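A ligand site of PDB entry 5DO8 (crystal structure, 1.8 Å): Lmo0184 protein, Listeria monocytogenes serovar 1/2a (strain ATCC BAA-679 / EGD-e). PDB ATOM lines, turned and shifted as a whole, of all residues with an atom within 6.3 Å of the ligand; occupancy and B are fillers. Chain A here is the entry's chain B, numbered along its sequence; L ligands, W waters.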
ATOM      1  N   TRP A  50      17.082 -43.640  -9.574  1.00  0.00           N
ATOM      2  CA  TRP A  50      16.955 -42.279  -9.061  1.00  0.00           C
ATOM      3  C   TRP A  50      16.359 -41.449 -10.212  1.00  0.00           C
ATOM      4  O   TRP A  50      16.989 -41.286 -11.247  1.00  0.00           O
ATOM      5  CB  TRP A  50      18.293 -41.737  -8.514  1.00  0.00           C
ATOM      6  CG  TRP A  50      18.357 -40.215  -8.404  1.00  0.00           C
ATOM      7  CD1 TRP A  50      17.321 -39.343  -8.240  1.00  0.00           C
ATOM      8  CD2 TRP A  50      19.520 -39.413  -8.534  1.00  0.00           C
ATOM      9  NE1 TRP A  50      17.756 -38.052  -8.235  1.00  0.00           N
ATOM     10  CE2 TRP A  50      19.124 -38.064  -8.404  1.00  0.00           C
ATOM     11  CE3 TRP A  50      20.877 -39.707  -8.713  1.00  0.00           C
ATOM     12  CZ2 TRP A  50      20.016 -37.026  -8.498  1.00  0.00           C
ATOM     13  CZ3 TRP A  50      21.775 -38.654  -8.778  1.00  0.00           C
ATOM     14  CH2 TRP A  50      21.341 -37.333  -8.689  1.00  0.00           C
ATOM     15  N   ASP A  61      14.426 -24.279 -13.763  1.00  0.00           N
ATOM     16  CA  ASP A  61      15.591 -25.114 -13.489  1.00  0.00           C
ATOM     17  C   ASP A  61      15.229 -26.578 -13.720  1.00  0.00           C
ATOM     18  O   ASP A  61      15.591 -27.462 -12.938  1.00  0.00           O
ATOM     19  CB  ASP A  61      16.085 -24.869 -12.060  1.00  0.00           C
ATOM     20  CG  ASP A  61      17.470 -25.459 -11.788  1.00  0.00           C
ATOM     21  OD1 ASP A  61      18.227 -25.739 -12.726  1.00  0.00           O
ATOM     22  OD2 ASP A  61      17.803 -25.620 -10.599  1.00  0.00           O
ATOM     23  N   TYR A  64      13.761 -28.617 -10.688  1.00  0.00           N
ATOM     24  CA  TYR A  64      14.293 -28.332  -9.347  1.00  0.00           C
ATOM     25  C   TYR A  64      13.697 -27.025  -8.783  1.00  0.00           C
ATOM     26  O   TYR A  64      14.062 -26.583  -7.704  1.00  0.00           O
ATOM     27  CB  TYR A  64      15.823 -28.378  -9.330  1.00  0.00           C
ATOM     28  CG  TYR A  64      16.361 -29.793  -9.470  1.00  0.00           C
ATOM     29  CD1 TYR A  64      16.503 -30.638  -8.355  1.00  0.00           C
ATOM     30  CD2 TYR A  64      16.731 -30.300 -10.705  1.00  0.00           C
ATOM     31  CE1 TYR A  64      16.976 -31.938  -8.480  1.00  0.00           C
ATOM     32  CE2 TYR A  64      17.213 -31.597 -10.841  1.00  0.00           C
ATOM     33  CZ  TYR A  64      17.342 -32.408  -9.734  1.00  0.00           C
ATOM     34  OH  TYR A  64      17.802 -33.704  -9.870  1.00  0.00           O
ATOM     35  N   ASP A  65      12.788 -26.413  -9.555  1.00  0.00           N
ATOM     36  CA  ASP A  65      11.936 -25.320  -9.110  1.00  0.00           C
ATOM     37  C   ASP A  65      10.497 -25.815  -8.998  1.00  0.00           C
ATOM     38  O   ASP A  65       9.748 -25.773  -9.964  1.00  0.00           O
ATOM     39  CB  ASP A  65      12.077 -24.109 -10.041  1.00  0.00           C
ATOM     40  CG  ASP A  65      11.799 -24.414 -11.530  1.00  0.00           C
ATOM     41  OD1 ASP A  65      12.240 -25.446 -12.092  1.00  0.00           O
ATOM     42  OD2 ASP A  65      11.155 -23.560 -12.156  1.00  0.00           O
ATOM     43  N   ASP A  99      14.121 -36.995  -5.848  1.00  0.00           N
ATOM     44  CA  ASP A  99      14.741 -35.818  -5.259  1.00  0.00           C
ATOM     45  C   ASP A  99      13.791 -35.171  -4.271  1.00  0.00           C
ATOM     46  O   ASP A  99      12.604 -34.969  -4.559  1.00  0.00           O
ATOM     47  CB  ASP A  99      15.168 -34.795  -6.321  1.00  0.00           C
ATOM     48  CG  ASP A  99      16.499 -35.134  -6.961  1.00  0.00           C
ATOM     49  OD1 ASP A  99      17.563 -35.021  -6.310  1.00  0.00           O
ATOM     50  OD2 ASP A  99      16.512 -35.508  -8.132  1.00  0.00           O
ATOM     51  N   VAL A 101      13.458 -31.712  -2.779  1.00  0.00           N
ATOM     52  CA  VAL A 101      13.921 -30.387  -3.144  1.00  0.00           C
ATOM     53  C   VAL A 101      13.287 -29.396  -2.188  1.00  0.00           C
ATOM     54  O   VAL A 101      12.224 -28.846  -2.476  1.00  0.00           O
ATOM     55  CB  VAL A 101      13.541 -30.067  -4.611  1.00  0.00           C
ATOM     56  CG1 VAL A 101      14.197 -28.773  -5.065  1.00  0.00           C
ATOM     57  CG2 VAL A 101      13.939 -31.213  -5.548  1.00  0.00           C
ATOM     58  N   HIS A 104      14.356 -24.683  -1.423  1.00  0.00           N
ATOM     59  CA  HIS A 104      13.650 -23.650  -2.152  1.00  0.00           C
ATOM     60  C   HIS A 104      12.475 -24.248  -2.869  1.00  0.00           C
ATOM     61  O   HIS A 104      12.397 -25.471  -3.050  1.00  0.00           O
ATOM     62  CB  HIS A 104      14.592 -22.964  -3.172  1.00  0.00           C
ATOM     63  CG  HIS A 104      15.323 -23.923  -4.057  1.00  0.00           C
ATOM     64  ND1 HIS A 104      16.586 -24.385  -3.757  1.00  0.00           N
ATOM     65  CD2 HIS A 104      14.964 -24.540  -5.207  1.00  0.00           C
ATOM     66  CE1 HIS A 104      16.986 -25.217  -4.709  1.00  0.00           C
ATOM     67  NE2 HIS A 104      16.012 -25.330  -5.598  1.00  0.00           N
ATOM     68  N   PHE A 142      23.386 -18.957  -9.720  1.00  0.00           N
ATOM     69  CA  PHE A 142      23.075 -18.793 -11.145  1.00  0.00           C
ATOM     70  C   PHE A 142      23.201 -17.335 -11.628  1.00  0.00           C
ATOM     71  O   PHE A 142      22.425 -16.890 -12.480  1.00  0.00           O
ATOM     72  CB  PHE A 142      21.664 -19.335 -11.469  1.00  0.00           C
ATOM     73  CG  PHE A 142      21.483 -20.818 -11.247  1.00  0.00           C
ATOM     74  CD1 PHE A 142      22.571 -21.712 -11.196  1.00  0.00           C
ATOM     75  CD2 PHE A 142      20.187 -21.326 -11.136  1.00  0.00           C
ATOM     76  CE1 PHE A 142      22.356 -23.059 -11.022  1.00  0.00           C
ATOM     77  CE2 PHE A 142      19.989 -22.686 -10.962  1.00  0.00           C
ATOM     78  CZ  PHE A 142      21.065 -23.545 -10.890  1.00  0.00           C
ATOM     79  N   PHE A 161      19.548 -19.837  -5.811  1.00  0.00           N
ATOM     80  CA  PHE A 161      19.548 -20.263  -7.199  1.00  0.00           C
ATOM     81  C   PHE A 161      18.811 -19.221  -8.045  1.00  0.00           C
ATOM     82  O   PHE A 161      19.063 -18.030  -7.855  1.00  0.00           O
ATOM     83  CB  PHE A 161      19.052 -21.706  -7.295  1.00  0.00           C
ATOM     84  CG  PHE A 161      19.969 -22.679  -6.581  1.00  0.00           C
ATOM     85  CD1 PHE A 161      21.095 -23.180  -7.235  1.00  0.00           C
ATOM     86  CD2 PHE A 161      19.725 -23.062  -5.277  1.00  0.00           C
ATOM     87  CE1 PHE A 161      21.944 -24.083  -6.590  1.00  0.00           C
ATOM     88  CE2 PHE A 161      20.566 -23.939  -4.620  1.00  0.00           C
ATOM     89  CZ  PHE A 161      21.669 -24.462  -5.283  1.00  0.00           C
ATOM     90  N   GLN A 165      13.429 -19.304  -7.797  1.00  0.00           N
ATOM     91  CA  GLN A 165      13.662 -20.317  -6.777  1.00  0.00           C
ATOM     92  C   GLN A 165      13.899 -19.697  -5.386  1.00  0.00           C
ATOM     93  O   GLN A 165      15.013 -19.770  -4.860  1.00  0.00           O
ATOM     94  CB  GLN A 165      14.857 -21.180  -7.158  1.00  0.00           C
ATOM     95  CG  GLN A 165      14.562 -22.115  -8.324  1.00  0.00           C
ATOM     96  CD  GLN A 165      15.808 -22.779  -8.888  1.00  0.00           C
ATOM     97  OE1 GLN A 165      16.671 -22.109  -9.449  1.00  0.00           O
ATOM     98  NE2 GLN A 165      15.891 -24.086  -8.778  1.00  0.00           N
ATOM     99  N   ARG A 195      16.927 -38.450  -2.424  1.00  0.00           N
ATOM    100  CA  ARG A 195      18.174 -37.691  -2.444  1.00  0.00           C
ATOM    101  C   ARG A 195      17.796 -36.296  -1.964  1.00  0.00           C
ATOM    102  O   ARG A 195      16.944 -35.636  -2.551  1.00  0.00           O
ATOM    103  CB  ARG A 195      18.803 -37.603  -3.844  1.00  0.00           C
ATOM    104  CG  ARG A 195      20.231 -37.037  -3.790  1.00  0.00           C
ATOM    105  CD  ARG A 195      20.855 -36.824  -5.152  1.00  0.00           C
ATOM    106  NE  ARG A 195      20.330 -35.622  -5.790  1.00  0.00           N
ATOM    107  CZ  ARG A 195      21.030 -34.639  -6.351  1.00  0.00           C
ATOM    108  NH1 ARG A 195      20.369 -33.630  -6.910  1.00  0.00           N
ATOM    109  NH2 ARG A 195      22.352 -34.656  -6.428  1.00  0.00           N
ATOM    110  N   MET A 196      18.426 -35.863  -0.871  1.00  0.00           N
ATOM    111  CA  MET A 196      18.082 -34.575  -0.258  1.00  0.00           C
ATOM    112  C   MET A 196      18.988 -33.531  -0.847  1.00  0.00           C
ATOM    113  O   MET A 196      20.190 -33.481  -0.537  1.00  0.00           O
ATOM    114  CB  MET A 196      18.218 -34.661   1.258  1.00  0.00           C
ATOM    115  CG  MET A 196      17.374 -35.757   1.852  1.00  0.00           C
ATOM    116  SD  MET A 196      17.367 -35.657   3.634  1.00  0.00           S
ATOM    117  CE  MET A 196      16.472 -37.164   4.039  1.00  0.00           C
ATOM    118  N   ASP A 197      18.402 -32.703  -1.707  1.00  0.00           N
ATOM    119  CA  ASP A 197      19.138 -31.744  -2.501  1.00  0.00           C
ATOM    120  C   ASP A 197      19.685 -30.582  -1.674  1.00  0.00           C
ATOM    121  O   ASP A 197      18.947 -30.003  -0.866  1.00  0.00           O
ATOM    122  CB  ASP A 197      18.247 -31.189  -3.608  1.00  0.00           C
ATOM    123  CG  ASP A 197      17.752 -32.259  -4.540  1.00  0.00           C
ATOM    124  OD1 ASP A 197      18.033 -33.457  -4.355  1.00  0.00           O
ATOM    125  OD2 ASP A 197      17.030 -31.876  -5.454  1.00  0.00           O
ATOM    126  N   VAL A 198      20.959 -30.278  -1.900  1.00  0.00           N
ATOM    127  CA  VAL A 198      21.727 -29.243  -1.199  1.00  0.00           C
ATOM    128  C   VAL A 198      21.240 -29.062   0.237  1.00  0.00           C
ATOM    129  O   VAL A 198      20.949 -27.948   0.694  1.00  0.00           O
ATOM    130  CB  VAL A 198      21.759 -27.914  -2.001  1.00  0.00           C
ATOM    131  CG1 VAL A 198      22.522 -28.123  -3.315  1.00  0.00           C
ATOM    132  CG2 VAL A 198      20.371 -27.402  -2.320  1.00  0.00           C
ATOM    133  N   GLU A 254      22.941 -34.693  -0.358  1.00  0.00           N
ATOM    134  CA  GLU A 254      23.761 -33.920  -1.306  1.00  0.00           C
ATOM    135  C   GLU A 254      24.252 -32.693  -0.569  1.00  0.00           C
ATOM    136  O   GLU A 254      23.460 -31.824  -0.217  1.00  0.00           O
ATOM    137  CB  GLU A 254      22.939 -33.513  -2.529  1.00  0.00           C
ATOM    138  CG  GLU A 254      23.749 -32.801  -3.619  1.00  0.00           C
ATOM    139  CD  GLU A 254      22.923 -31.956  -4.585  1.00  0.00           C
ATOM    140  OE1 GLU A 254      21.872 -31.439  -4.222  1.00  0.00           O
ATOM    141  OE2 GLU A 254      23.356 -31.756  -5.749  1.00  0.00           O
ATOM    142  N   ASN A 326      26.410 -36.984 -13.535  1.00  0.00           N
ATOM    143  CA  ASN A 326      24.979 -36.856 -13.321  1.00  0.00           C
ATOM    144  C   ASN A 326      24.509 -35.684 -14.169  1.00  0.00           C
ATOM    145  O   ASN A 326      25.261 -35.155 -14.990  1.00  0.00           O
ATOM    146  CB  ASN A 326      24.683 -36.662 -11.819  1.00  0.00           C
ATOM    147  CG  ASN A 326      25.466 -35.536 -11.226  1.00  0.00           C
ATOM    148  OD1 ASN A 326      25.520 -34.441 -11.767  1.00  0.00           O
ATOM    149  ND2 ASN A 326      26.126 -35.812 -10.110  1.00  0.00           N
ATOM    150  N   HIS A 327      23.262 -35.285 -13.988  1.00  0.00           N
ATOM    151  CA  HIS A 327      22.661 -34.162 -14.715  1.00  0.00           C
ATOM    152  C   HIS A 327      23.303 -32.767 -14.486  1.00  0.00           C
ATOM    153  O   HIS A 327      22.941 -31.824 -15.182  1.00  0.00           O
ATOM    154  CB  HIS A 327      21.175 -34.071 -14.369  1.00  0.00           C
ATOM    155  CG  HIS A 327      20.939 -33.664 -12.954  1.00  0.00           C
ATOM    156  ND1 HIS A 327      21.364 -34.394 -11.871  1.00  0.00           N
ATOM    157  CD2 HIS A 327      20.377 -32.541 -12.442  1.00  0.00           C
ATOM    158  CE1 HIS A 327      21.050 -33.774 -10.750  1.00  0.00           C
ATOM    159  NE2 HIS A 327      20.450 -32.647 -11.069  1.00  0.00           N
ATOM    160  N   ASP A 328      24.230 -32.677 -13.520  1.00  0.00           N
ATOM    161  CA  ASP A 328      24.947 -31.440 -13.237  1.00  0.00           C
ATOM    162  C   ASP A 328      26.412 -31.435 -13.699  1.00  0.00           C
ATOM    163  O   ASP A 328      27.090 -30.448 -13.503  1.00  0.00           O
ATOM    164  CB  ASP A 328      24.958 -31.150 -11.716  1.00  0.00           C
ATOM    165  CG  ASP A 328      23.593 -30.813 -11.162  1.00  0.00           C
ATOM    166  OD1 ASP A 328      22.751 -30.252 -11.886  1.00  0.00           O
ATOM    167  OD2 ASP A 328      23.420 -31.055  -9.931  1.00  0.00           O
ATOM    168  N   ARG A 413      26.176 -27.991 -17.962  1.00  0.00           N
ATOM    169  CA  ARG A 413      25.292 -29.090 -17.580  1.00  0.00           C
ATOM    170  C   ARG A 413      24.547 -29.710 -18.783  1.00  0.00           C
ATOM    171  O   ARG A 413      24.153 -30.867 -18.729  1.00  0.00           O
ATOM    172  CB  ARG A 413      24.320 -28.637 -16.486  1.00  0.00           C
ATOM    173  CG  ARG A 413      25.055 -28.183 -15.235  1.00  0.00           C
ATOM    174  CD  ARG A 413      24.120 -27.992 -14.047  1.00  0.00           C
ATOM    175  NE  ARG A 413      23.092 -26.982 -14.265  1.00  0.00           N
ATOM    176  CZ  ARG A 413      22.117 -26.697 -13.390  1.00  0.00           C
ATOM    177  NH1 ARG A 413      22.060 -27.330 -12.206  1.00  0.00           N
ATOM    178  NH2 ARG A 413      21.201 -25.777 -13.669  1.00  0.00           N
ATOM    179  N   ARG A 417      22.564 -33.555 -20.616  1.00  0.00           N
ATOM    180  CA  ARG A 417      21.127 -33.468 -20.817  1.00  0.00           C
ATOM    181  C   ARG A 417      20.686 -33.681 -22.257  1.00  0.00           C
ATOM    182  O   ARG A 417      19.462 -33.728 -22.536  1.00  0.00           O
ATOM    183  CB  ARG A 417      20.673 -32.110 -20.288  1.00  0.00           C
ATOM    184  CG  ARG A 417      20.940 -31.951 -18.801  1.00  0.00           C
ATOM    185  CD  ARG A 417      20.647 -30.535 -18.329  1.00  0.00           C
ATOM    186  NE  ARG A 417      20.954 -30.449 -16.899  1.00  0.00           N
ATOM    187  CZ  ARG A 417      20.511 -29.514 -16.070  1.00  0.00           C
ATOM    188  NH1 ARG A 417      19.717 -28.514 -16.496  1.00  0.00           N
ATOM    189  NH2 ARG A 417      20.860 -29.566 -14.775  1.00  0.00           N
HETATM  190  C1  LIG L   1      20.392 -30.144  -8.419  1.00  0.00           C
HETATM  191  C2  LIG L   1      20.680 -29.110  -9.497  1.00  0.00           C
HETATM  192  C3  LIG L   1      19.821 -27.880  -9.238  1.00  0.00           C
HETATM  193  C4  LIG L   1      20.075 -27.361  -7.820  1.00  0.00           C
HETATM  194  C5  LIG L   1      19.191 -26.173  -7.464  1.00  0.00           C
HETATM  195  C6  LIG L   1      20.668 -29.554  -7.044  1.00  0.00           C
HETATM  196  O1  LIG L   1      20.370 -30.499  -6.019  1.00  0.00           O
HETATM  197  O2  LIG L   1      21.155 -31.338  -8.640  1.00  0.00           O
HETATM  198  O3  LIG L   1      20.412 -29.674 -10.791  1.00  0.00           O
HETATM  199  O4  LIG L   1      20.095 -26.870 -10.213  1.00  0.00           O
HETATM  200  O5  LIG L   1      19.867 -28.395  -6.856  1.00  0.00           O
HETATM  201  O6  LIG L   1      17.828 -26.562  -7.557  1.00  0.00           O
HETATM  202  O   HOH W   1      17.676 -28.487  -5.214  1.00  0.00           O
HETATM  203  O   HOH W   2      19.109 -28.499 -12.810  1.00  0.00           O
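An oxygen (O1) of the ligand sits at hydrogen-bond distance from the side-chain carboxylate (OE1) of Glu 254 (2.5 Å).
O4 of the ligand is in hydrogen-bond range of OD2 of Asp 61.
A ring nitrogen (NE2) of His 104 sits at hydrogen-bond distance from an oxygen (O6) of the ligand, 2.9 Å away.
O2 of the ligand sits at hydrogen-bond distance from NE2 of His 327 (2.8 Å).
The guanidinium group of Arg 195 sits at hydrogen-bond distance from an oxygen (O2) of the ligand, at 3.0 Å.
The guanidinium group (NH1) of Arg 413 sits at hydrogen-bond distance from an oxygen (O4) of the ligand, at 2.8 Å.
O2 of the ligand is in hydrogen-bond range of OD2 of Asp 328, 2.6 Å away.
The side-chain amide nitrogen (NE2) of Gln 165 lies within hydrogen-bond range of an oxygen (O6) of the ligand (3.4 Å).
Merely in contact with the ligand: Tyr 64, Phe 142, Phe 161 and Asp 197.
Hydrophobic or aromatic side chains that line the ligand: Tyr 64, His 104, Phe 142, Phe 161 and His 327.
Within 4 Å of the ligand: Asp 61, Tyr 64, His 104, Phe 142, Phe 161, Gln 165, Arg 195, Asp 197, Glu 254, His 327, Asp 328 and Arg 413.
The nearest printed residue that does not touch the ligand is Arg 417 (4.01 Å).
NH2 of Arg 413 is in salt-bridge range of OD1 of Asp 61 (3.1 Å).
OE1 of Glu 254 sits at hydrogen-bond distance from N of Val 198 (2.8 Å).
OD2 of Asp 99 sits at hydrogen-bond distance from OH of Tyr 64, at 2.8 Å.
The guanidinium group (NH1) of Arg 195 is in salt-bridge range of the side-chain carboxylate (OD1) of Asp 197 (3.5 Å).
The backbone NH (N) of Asp 328 is in hydrogen-bond range of the side-chain amide oxygen (OD1) of Asn 326, 2.8 Å away.
OD1 of Asp 99 is in salt-bridge range of NE of Arg 195.
The side-chain carboxylate (OE2) of Glu 254 lies within salt-bridge range of the guanidinium group (NH2) of Arg 195, at 3.1 Å.
The backbone carbonyl oxygen (O) of Met 196 sits at hydrogen-bond distance from the backbone NH (N) of Glu 254, at 3.0 Å.
Water W2 lies within hydrogen-bond range of O3 of the ligand (2.7 Å), NH2 of Arg 417 (2.8 Å), OD1 of Asp 61 (2.9 Å) and NH1 of Arg 413 (3.2 Å).
Water W1 bridges O5 of the ligand (2.7 Å) and OD2 of Asp 197 (3.5 Å).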
